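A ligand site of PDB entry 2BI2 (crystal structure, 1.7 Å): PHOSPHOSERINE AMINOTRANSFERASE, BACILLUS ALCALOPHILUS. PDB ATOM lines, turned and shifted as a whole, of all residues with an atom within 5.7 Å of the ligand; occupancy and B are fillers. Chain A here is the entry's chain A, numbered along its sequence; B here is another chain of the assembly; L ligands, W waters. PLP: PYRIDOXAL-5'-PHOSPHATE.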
ATOM      1  N   GLY A  74       8.270  10.573  -3.296  1.00  0.00           N
ATOM      2  CA  GLY A  74       8.123  12.026  -3.314  1.00  0.00           C
ATOM      3  C   GLY A  74       7.686  12.569  -4.651  1.00  0.00           C
ATOM      4  O   GLY A  74       7.308  13.749  -4.731  1.00  0.00           O
ATOM      5  N   GLY A  75       7.738  11.749  -5.689  1.00  0.00           N
ATOM      6  CA  GLY A  75       7.271  12.232  -6.982  1.00  0.00           C
ATOM      7  C   GLY A  75       8.325  13.080  -7.676  1.00  0.00           C
ATOM      8  O   GLY A  75       9.377  13.425  -7.125  1.00  0.00           O
ATOM      9  N   ALA A  76       8.012  13.426  -8.932  1.00  0.00           N
ATOM     10  CA  ALA A  76       8.956  14.303  -9.637  1.00  0.00           C
ATOM     11  C   ALA A  76       9.019  15.635  -8.924  1.00  0.00           C
ATOM     12  O   ALA A  76      10.022  16.350  -8.882  1.00  0.00           O
ATOM     13  CB  ALA A  76       8.513  14.458 -11.091  1.00  0.00           C
ATOM     14  N   SER A  77       7.888  15.982  -8.322  1.00  0.00           N
ATOM     15  CA  SER A  77       7.829  17.261  -7.630  1.00  0.00           C
ATOM     16  C   SER A  77       8.876  17.366  -6.536  1.00  0.00           C
ATOM     17  O   SER A  77       9.441  18.443  -6.389  1.00  0.00           O
ATOM     18  CB  SER A  77       6.451  17.540  -7.024  1.00  0.00           C
ATOM     19  OG  SER A  77       5.522  17.690  -8.084  1.00  0.00           O
ATOM     20  N   LEU A  78       9.150  16.285  -5.806  1.00  0.00           N
ATOM     21  CA  LEU A  78      10.196  16.390  -4.800  1.00  0.00           C
ATOM     22  C   LEU A  78      11.566  16.551  -5.480  1.00  0.00           C
ATOM     23  O   LEU A  78      12.474  17.183  -4.938  1.00  0.00           O
ATOM     24  CB  LEU A  78      10.222  15.173  -3.868  1.00  0.00           C
ATOM     25  CG  LEU A  78      11.241  15.275  -2.733  1.00  0.00           C
ATOM     26  CD1 LEU A  78      10.980  16.528  -1.905  1.00  0.00           C
ATOM     27  CD2 LEU A  78      11.237  14.032  -1.856  1.00  0.00           C
ATOM     28  N   PHE A  80      12.162  18.338  -8.011  1.00  0.00           N
ATOM     29  CA  PHE A  80      12.315  19.763  -8.326  1.00  0.00           C
ATOM     30  C   PHE A  80      13.119  20.488  -7.257  1.00  0.00           C
ATOM     31  O   PHE A  80      13.881  21.416  -7.557  1.00  0.00           O
ATOM     32  CB  PHE A  80      10.958  20.435  -8.477  1.00  0.00           C
ATOM     33  CG  PHE A  80      10.082  20.018  -9.646  1.00  0.00           C
ATOM     34  CD1 PHE A  80       8.724  20.336  -9.632  1.00  0.00           C
ATOM     35  CD2 PHE A  80      10.609  19.319 -10.728  1.00  0.00           C
ATOM     36  CE1 PHE A  80       7.893  19.971 -10.686  1.00  0.00           C
ATOM     37  CE2 PHE A  80       9.796  18.978 -11.780  1.00  0.00           C
ATOM     38  CZ  PHE A  80       8.438  19.296 -11.767  1.00  0.00           C
ATOM     39  N   TRP A 102       5.316  22.256 -16.357  1.00  0.00           N
ATOM     40  CA  TRP A 102       6.218  21.500 -15.494  1.00  0.00           C
ATOM     41  C   TRP A 102       7.613  22.113 -15.482  1.00  0.00           C
ATOM     42  O   TRP A 102       8.281  22.104 -14.449  1.00  0.00           O
ATOM     43  CB  TRP A 102       6.280  20.011 -15.857  1.00  0.00           C
ATOM     44  CG  TRP A 102       4.962  19.348 -15.572  1.00  0.00           C
ATOM     45  CD1 TRP A 102       4.082  18.786 -16.441  1.00  0.00           C
ATOM     46  CD2 TRP A 102       4.389  19.178 -14.273  1.00  0.00           C
ATOM     47  NE1 TRP A 102       2.992  18.288 -15.789  1.00  0.00           N
ATOM     48  CE2 TRP A 102       3.162  18.513 -14.437  1.00  0.00           C
ATOM     49  CE3 TRP A 102       4.810  19.519 -12.979  1.00  0.00           C
ATOM     50  CZ2 TRP A 102       2.333  18.178 -13.359  1.00  0.00           C
ATOM     51  CZ3 TRP A 102       3.976  19.187 -11.931  1.00  0.00           C
ATOM     52  CH2 TRP A 102       2.756  18.535 -12.109  1.00  0.00           C
ATOM     53  N   THR A 148      12.740  19.763 -19.675  1.00  0.00           N
ATOM     54  CA  THR A 148      11.574  18.886 -19.557  1.00  0.00           C
ATOM     55  C   THR A 148      11.407  18.179 -20.903  1.00  0.00           C
ATOM     56  O   THR A 148      10.989  18.799 -21.885  1.00  0.00           O
ATOM     57  CB  THR A 148      10.334  19.685 -19.154  1.00  0.00           C
ATOM     58  OG1 THR A 148      10.719  20.537 -18.058  1.00  0.00           O
ATOM     59  CG2 THR A 148       9.194  18.775 -18.691  1.00  0.00           C
ATOM     60  N   ASN A 150       9.373  15.931 -22.180  1.00  0.00           N
ATOM     61  CA  ASN A 150       7.993  15.872 -22.671  1.00  0.00           C
ATOM     62  C   ASN A 150       7.123  16.785 -21.821  1.00  0.00           C
ATOM     63  O   ASN A 150       7.043  16.598 -20.584  1.00  0.00           O
ATOM     64  CB  ASN A 150       7.449  14.431 -22.680  1.00  0.00           C
ATOM     65  CG  ASN A 150       6.084  14.341 -23.323  1.00  0.00           C
ATOM     66  OD1 ASN A 150       5.037  14.307 -22.684  1.00  0.00           O
ATOM     67  ND2 ASN A 150       6.049  14.322 -24.649  1.00  0.00           N
ATOM     68  N   ASN A 151       6.506  17.775 -22.457  1.00  0.00           N
ATOM     69  CA  ASN A 151       5.739  18.792 -21.735  1.00  0.00           C
ATOM     70  C   ASN A 151       4.290  18.353 -21.670  1.00  0.00           C
ATOM     71  O   ASN A 151       3.485  18.625 -22.556  1.00  0.00           O
ATOM     72  CB  ASN A 151       5.942  20.150 -22.436  1.00  0.00           C
ATOM     73  CG  ASN A 151       7.428  20.419 -22.553  1.00  0.00           C
ATOM     74  OD1 ASN A 151       8.060  20.845 -21.570  1.00  0.00           O
ATOM     75  ND2 ASN A 151       8.012  20.166 -23.716  1.00  0.00           N
ATOM     76  N   THR A 152       4.025  17.633 -20.568  1.00  0.00           N
ATOM     77  CA  THR A 152       2.827  16.831 -20.411  1.00  0.00           C
ATOM     78  C   THR A 152       1.548  17.607 -20.672  1.00  0.00           C
ATOM     79  O   THR A 152       0.549  17.107 -21.196  1.00  0.00           O
ATOM     80  CB  THR A 152       2.785  16.238 -18.994  1.00  0.00           C
ATOM     81  OG1 THR A 152       4.133  15.914 -18.656  1.00  0.00           O
ATOM     82  CG2 THR A 152       2.002  14.933 -18.952  1.00  0.00           C
ATOM     83  N   ASP A 172      13.741  16.265 -16.633  1.00  0.00           N
ATOM     84  CA  ASP A 172      12.464  15.734 -16.147  1.00  0.00           C
ATOM     85  C   ASP A 172      11.826  14.949 -17.292  1.00  0.00           C
ATOM     86  O   ASP A 172      11.211  15.540 -18.195  1.00  0.00           O
ATOM     87  CB  ASP A 172      11.558  16.848 -15.665  1.00  0.00           C
ATOM     88  CG  ASP A 172      10.190  16.402 -15.218  1.00  0.00           C
ATOM     89  OD1 ASP A 172       9.929  15.173 -15.254  1.00  0.00           O
ATOM     90  OD2 ASP A 172       9.400  17.302 -14.834  1.00  0.00           O
ATOM     91  N   MET A 173      11.969  13.618 -17.236  1.00  0.00           N
ATOM     92  CA  MET A 173      11.373  12.788 -18.285  1.00  0.00           C
ATOM     93  C   MET A 173      10.126  12.042 -17.810  1.00  0.00           C
ATOM     94  O   MET A 173       9.864  10.989 -18.379  1.00  0.00           O
ATOM     95  CB  MET A 173      12.404  11.778 -18.783  1.00  0.00           C
ATOM     96  CG  MET A 173      13.624  12.449 -19.428  1.00  0.00           C
ATOM     97  SD  MET A 173      14.606  11.205 -20.297  1.00  0.00           S
ATOM     98  CE  MET A 173      15.843  12.274 -21.073  1.00  0.00           C
ATOM     99  N   SER A 174       9.419  12.563 -16.822  1.00  0.00           N
ATOM    100  CA  SER A 174       8.256  11.886 -16.240  1.00  0.00           C
ATOM    101  C   SER A 174       7.326  11.316 -17.302  1.00  0.00           C
ATOM    102  O   SER A 174       6.898  10.159 -17.193  1.00  0.00           O
ATOM    103  CB  SER A 174       7.495  12.860 -15.353  1.00  0.00           C
ATOM    104  OG  SER A 174       8.282  13.295 -14.241  1.00  0.00           O
ATOM    105  N   SER A 175       7.001  12.114 -18.348  1.00  0.00           N
ATOM    106  CA  SER A 175       5.948  11.597 -19.232  1.00  0.00           C
ATOM    107  C   SER A 175       6.449  10.991 -20.518  1.00  0.00           C
ATOM    108  O   SER A 175       5.589  10.672 -21.369  1.00  0.00           O
ATOM    109  CB  SER A 175       4.903  12.706 -19.506  1.00  0.00           C
ATOM    110  OG  SER A 175       5.546  13.914 -19.867  1.00  0.00           O
ATOM    111  N   GLY A 193       8.593  10.582 -12.322  1.00  0.00           N
ATOM    112  CA  GLY A 193       7.613   9.856 -11.508  1.00  0.00           C
ATOM    113  C   GLY A 193       7.224   8.626 -12.318  1.00  0.00           C
ATOM    114  O   GLY A 193       7.056   8.661 -13.543  1.00  0.00           O
ATOM    115  N   GLN A 195       4.407   7.005 -12.531  1.00  0.00           N
ATOM    116  CA  GLN A 195       2.989   6.848 -12.813  1.00  0.00           C
ATOM    117  C   GLN A 195       2.574   7.291 -14.203  1.00  0.00           C
ATOM    118  O   GLN A 195       1.415   7.207 -14.594  1.00  0.00           O
ATOM    119  CB  GLN A 195       2.137   7.624 -11.805  1.00  0.00           C
ATOM    120  CG  GLN A 195       2.294   9.148 -11.926  1.00  0.00           C
ATOM    121  CD  GLN A 195       3.387   9.685 -11.032  1.00  0.00           C
ATOM    122  OE1 GLN A 195       4.310   8.976 -10.622  1.00  0.00           O
ATOM    123  NE2 GLN A 195       3.331  10.982 -10.742  1.00  0.00           N
ATOM    124  N   LYS A 196       3.527   7.801 -14.999  1.00  0.00           N
ATOM    125  CA  LYS A 196       3.000   8.140 -16.339  1.00  0.00           C
ATOM    126  C   LYS A 196       3.294   7.038 -17.315  1.00  0.00           C
ATOM    127  O   LYS A 196       2.446   6.538 -18.054  1.00  0.00           O
ATOM    128  CB  LYS A 196       3.543   9.485 -16.811  1.00  0.00           C
ATOM    129  CG  LYS A 196       3.486  10.593 -15.769  1.00  0.00           C
ATOM    130  CD  LYS A 196       2.575  11.704 -16.235  1.00  0.00           C
ATOM    131  CE  LYS A 196       2.040  12.524 -15.074  1.00  0.00           C
ATOM    132  NZ  LYS A 196       2.852  13.763 -14.887  1.00  0.00           N
ATOM    133  N   THR A 204       9.618   7.187  -7.752  1.00  0.00           N
ATOM    134  CA  THR A 204      10.223   8.086  -8.722  1.00  0.00           C
ATOM    135  C   THR A 204      11.564   7.493  -9.159  1.00  0.00           C
ATOM    136  O   THR A 204      12.372   7.190  -8.285  1.00  0.00           O
ATOM    137  CB  THR A 204      10.406   9.480  -8.095  1.00  0.00           C
ATOM    138  OG1 THR A 204       9.101  10.018  -7.836  1.00  0.00           O
ATOM    139  CG2 THR A 204      11.131  10.408  -9.051  1.00  0.00           C
ATOM    140  N   TYR A 338       0.537   7.056 -23.537  1.00  0.00           N
ATOM    141  CA  TYR A 338       1.760   6.431 -23.032  1.00  0.00           C
ATOM    142  C   TYR A 338       1.935   4.993 -23.537  1.00  0.00           C
ATOM    143  O   TYR A 338       0.990   4.479 -24.134  1.00  0.00           O
ATOM    144  CB  TYR A 338       1.688   6.425 -21.492  1.00  0.00           C
ATOM    145  CG  TYR A 338       1.516   7.798 -20.899  1.00  0.00           C
ATOM    146  CD1 TYR A 338       0.394   8.109 -20.138  1.00  0.00           C
ATOM    147  CD2 TYR A 338       2.475   8.775 -21.071  1.00  0.00           C
ATOM    148  CE1 TYR A 338       0.231   9.356 -19.571  1.00  0.00           C
ATOM    149  CE2 TYR A 338       2.319  10.035 -20.518  1.00  0.00           C
ATOM    150  CZ  TYR A 338       1.206  10.331 -19.766  1.00  0.00           C
ATOM    151  OH  TYR A 338       1.013  11.583 -19.194  1.00  0.00           O
ATOM    152  N   HIS B  41      -5.354  10.756 -10.206  1.00  0.00           N
ATOM    153  CA  HIS B  41      -5.607  11.153  -8.817  1.00  0.00           C
ATOM    154  C   HIS B  41      -6.578  12.319  -8.755  1.00  0.00           C
ATOM    155  O   HIS B  41      -7.028  12.734  -7.694  1.00  0.00           O
ATOM    156  CB  HIS B  41      -4.287  11.497  -8.135  1.00  0.00           C
ATOM    157  CG  HIS B  41      -3.552  12.630  -8.781  1.00  0.00           C
ATOM    158  ND1 HIS B  41      -3.109  12.627 -10.087  1.00  0.00           N
ATOM    159  CD2 HIS B  41      -3.200  13.842  -8.267  1.00  0.00           C
ATOM    160  CE1 HIS B  41      -2.512  13.769 -10.343  1.00  0.00           C
ATOM    161  NE2 HIS B  41      -2.549  14.527  -9.254  1.00  0.00           N
ATOM    162  N   GLN B  73       4.442  11.132   1.113  1.00  0.00           N
ATOM    163  CA  GLN B  73       5.482  10.190   0.756  1.00  0.00           C
ATOM    164  C   GLN B  73       6.749  10.455   1.556  1.00  0.00           C
ATOM    165  O   GLN B  73       6.833  11.532   2.160  1.00  0.00           O
ATOM    166  CB  GLN B  73       5.798  10.297  -0.758  1.00  0.00           C
ATOM    167  CG  GLN B  73       4.590   9.973  -1.641  1.00  0.00           C
ATOM    168  CD  GLN B  73       4.985  10.001  -3.117  1.00  0.00           C
ATOM    169  OE1 GLN B  73       5.790   9.147  -3.538  1.00  0.00           O
ATOM    170  NE2 GLN B  73       4.451  10.969  -3.848  1.00  0.00           N
ATOM    171  N   ASN B 237       0.615  17.124  -5.325  1.00  0.00           N
ATOM    172  CA  ASN B 237       1.212  16.349  -6.429  1.00  0.00           C
ATOM    173  C   ASN B 237       0.572  14.964  -6.390  1.00  0.00           C
ATOM    174  O   ASN B 237      -0.394  14.746  -5.649  1.00  0.00           O
ATOM    175  CB  ASN B 237       2.725  16.281  -6.425  1.00  0.00           C
ATOM    176  CG  ASN B 237       3.331  15.381  -5.377  1.00  0.00           C
ATOM    177  OD1 ASN B 237       2.790  15.283  -4.271  1.00  0.00           O
ATOM    178  ND2 ASN B 237       4.432  14.734  -5.736  1.00  0.00           N
ATOM    179  N   THR B 238       1.053  14.054  -7.197  1.00  0.00           N
ATOM    180  CA  THR B 238       0.387  12.757  -7.308  1.00  0.00           C
ATOM    181  C   THR B 238       0.642  11.986  -6.010  1.00  0.00           C
ATOM    182  O   THR B 238       1.799  11.760  -5.661  1.00  0.00           O
ATOM    183  CB  THR B 238       0.928  11.960  -8.503  1.00  0.00           C
ATOM    184  OG1 THR B 238       0.929  12.767  -9.699  1.00  0.00           O
ATOM    185  CG2 THR B 238       0.034  10.760  -8.796  1.00  0.00           C
HETATM  186  N1  PLP L   1       6.882  16.558 -14.261  1.00  0.00           N
HETATM  187  C2  PLP L   1       6.210  16.109 -15.358  1.00  0.00           C
HETATM  188  C2A PLP L   1       6.781  16.303 -16.766  1.00  0.00           C
HETATM  189  C3  PLP L   1       5.017  15.458 -15.203  1.00  0.00           C
HETATM  190  O3  PLP L   1       4.362  15.089 -16.348  1.00  0.00           O
HETATM  191  C4  PLP L   1       4.520  15.299 -13.928  1.00  0.00           C
HETATM  192  C4A PLP L   1       3.265  14.420 -13.682  1.00  0.00           C
HETATM  193  C5  PLP L   1       5.170  15.803 -12.835  1.00  0.00           C
HETATM  194  C6  PLP L   1       6.367  16.447 -12.995  1.00  0.00           C
HETATM  195  C5A PLP L   1       4.596  15.640 -11.414  1.00  0.00           C
HETATM  196  O4P PLP L   1       4.972  14.390 -10.848  1.00  0.00           O
HETATM  197  P   PLP L   1       4.527  14.059  -9.345  1.00  0.00           P
HETATM  198  O1P PLP L   1       3.069  14.273  -9.332  1.00  0.00           O
HETATM  199  O2P PLP L   1       5.295  15.039  -8.536  1.00  0.00           O
HETATM  200  O3P PLP L   1       4.944  12.661  -9.128  1.00  0.00           O
HETATM  201  O   HOH W   1       4.182  11.410  -6.865  1.00  0.00           O
HETATM  202  O   HOH W   2       0.099  14.837 -13.224  1.00  0.00           O
HETATM  203  O   HOH W   3       1.520  16.546  -9.662  1.00  0.00           O
HETATM  204  O   HOH W   4       6.176  12.365 -12.461  1.00  0.00           O
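The side-chain hydroxyl (OG) of Ser 77 lies within hydrogen-bond range of an oxygen (O2P) of the ligand, 2.7 Å away.
NE2 of Gln 195 sits at hydrogen-bond distance from O3P of the ligand, at 2.8 Å.
An oxygen (O3P) of the ligand lies within hydrogen-bond range of the backbone NH of Ala 76, at 3.2 Å.
The side-chain carboxylate of Asp 172 sits at hydrogen-bond distance from a nitrogen (N1) of the ligand (2.7 Å).
The side-chain amide nitrogen (ND2) of Asn 237 of chain B sits at hydrogen-bond distance from an oxygen (O2P) of the ligand, 2.9 Å away.
A carbon (C4A) of the ligand is covalently linked to the side-chain amino group (NZ) of Lys 196 (1.4 Å).
N of Thr 238 of chain B sits at hydrogen-bond distance from O1P of the ligand, 2.9 Å away.
OG1 of Thr 238 of chain B is in hydrogen-bond range of O1P of the ligand, 2.6 Å away.
The side-chain hydroxyl of Thr 152 is in hydrogen-bond range of an oxygen (O3) of the ligand, at 2.5 Å.
O2P of the ligand sits at hydrogen-bond distance from N of Ser 77 (2.8 Å).
OG1 of Thr 238 of chain B is in hydrogen-bond range of NE2 of Gln 195 (3.2 Å).
The side-chain amide nitrogen (NE2) of Gln 73 of chain B is in hydrogen-bond range of the backbone carbonyl oxygen (O) of Thr 238 of chain B (3.3 Å).
OG of Ser 174 lies within hydrogen-bond range of N of Gly 193 (3.3 Å).
OD1 of Asn 150 lies within hydrogen-bond range of OG of Ser 175 (2.9 Å).
The side-chain hydroxyl of Ser 174 lies within hydrogen-bond range of the side-chain carboxylate of Asp 172 (2.7 Å).
The side-chain hydroxyl (OG1) of Thr 204 lies close to the backbone NH (N) of Gly 75, 3.1 Å away.
The side-chain amide nitrogen (ND2) of Asn 237 of chain B lies within hydrogen-bond range of the backbone carbonyl oxygen (O) of Gly 74.
The side-chain hydroxyl (OG1) of Thr 152 sits at hydrogen-bond distance from the side-chain hydroxyl (OG) of Ser 175, 2.7 Å away.
Residues that only touch the ligand: Gly 75 (3.2 Å), Trp 102 (3.4 Å), Ser 174 (3.5 Å), Phe 80 (3.7 Å), Asn 150 (3.8 Å), Ser 175 (3.9 Å) and Thr 148 (3.95 Å).
Hydrophobic or aromatic side chains that line the ligand: Ala 76, Phe 80 and Trp 102.
Within 4 Å of the ligand: Gly 75, Ala 76, Ser 77, Phe 80, Trp 102, Thr 148, Asn 150, Thr 152, Asp 172, Ser 174, Ser 175, Gln 195, Lys 196, Asn 237 of chain B and Thr 238 of chain B.
The nearest printed residue that does not touch the ligand is Gly 74 (4.5 Å).
Water W1 lies within hydrogen-bond range of O of Thr 238 of chain B (2.7 Å), O3P of the ligand (2.7 Å) and NE2 of Gln 73 of chain B (3.1 Å).
Water W4 lies within hydrogen-bond range of an oxygen (O4P) of the ligand (2.9 Å), the side-chain hydroxyl (OG) of Ser 174 (2.9 Å) and the backbone NH (N) of Gly 193 (3.0 Å).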
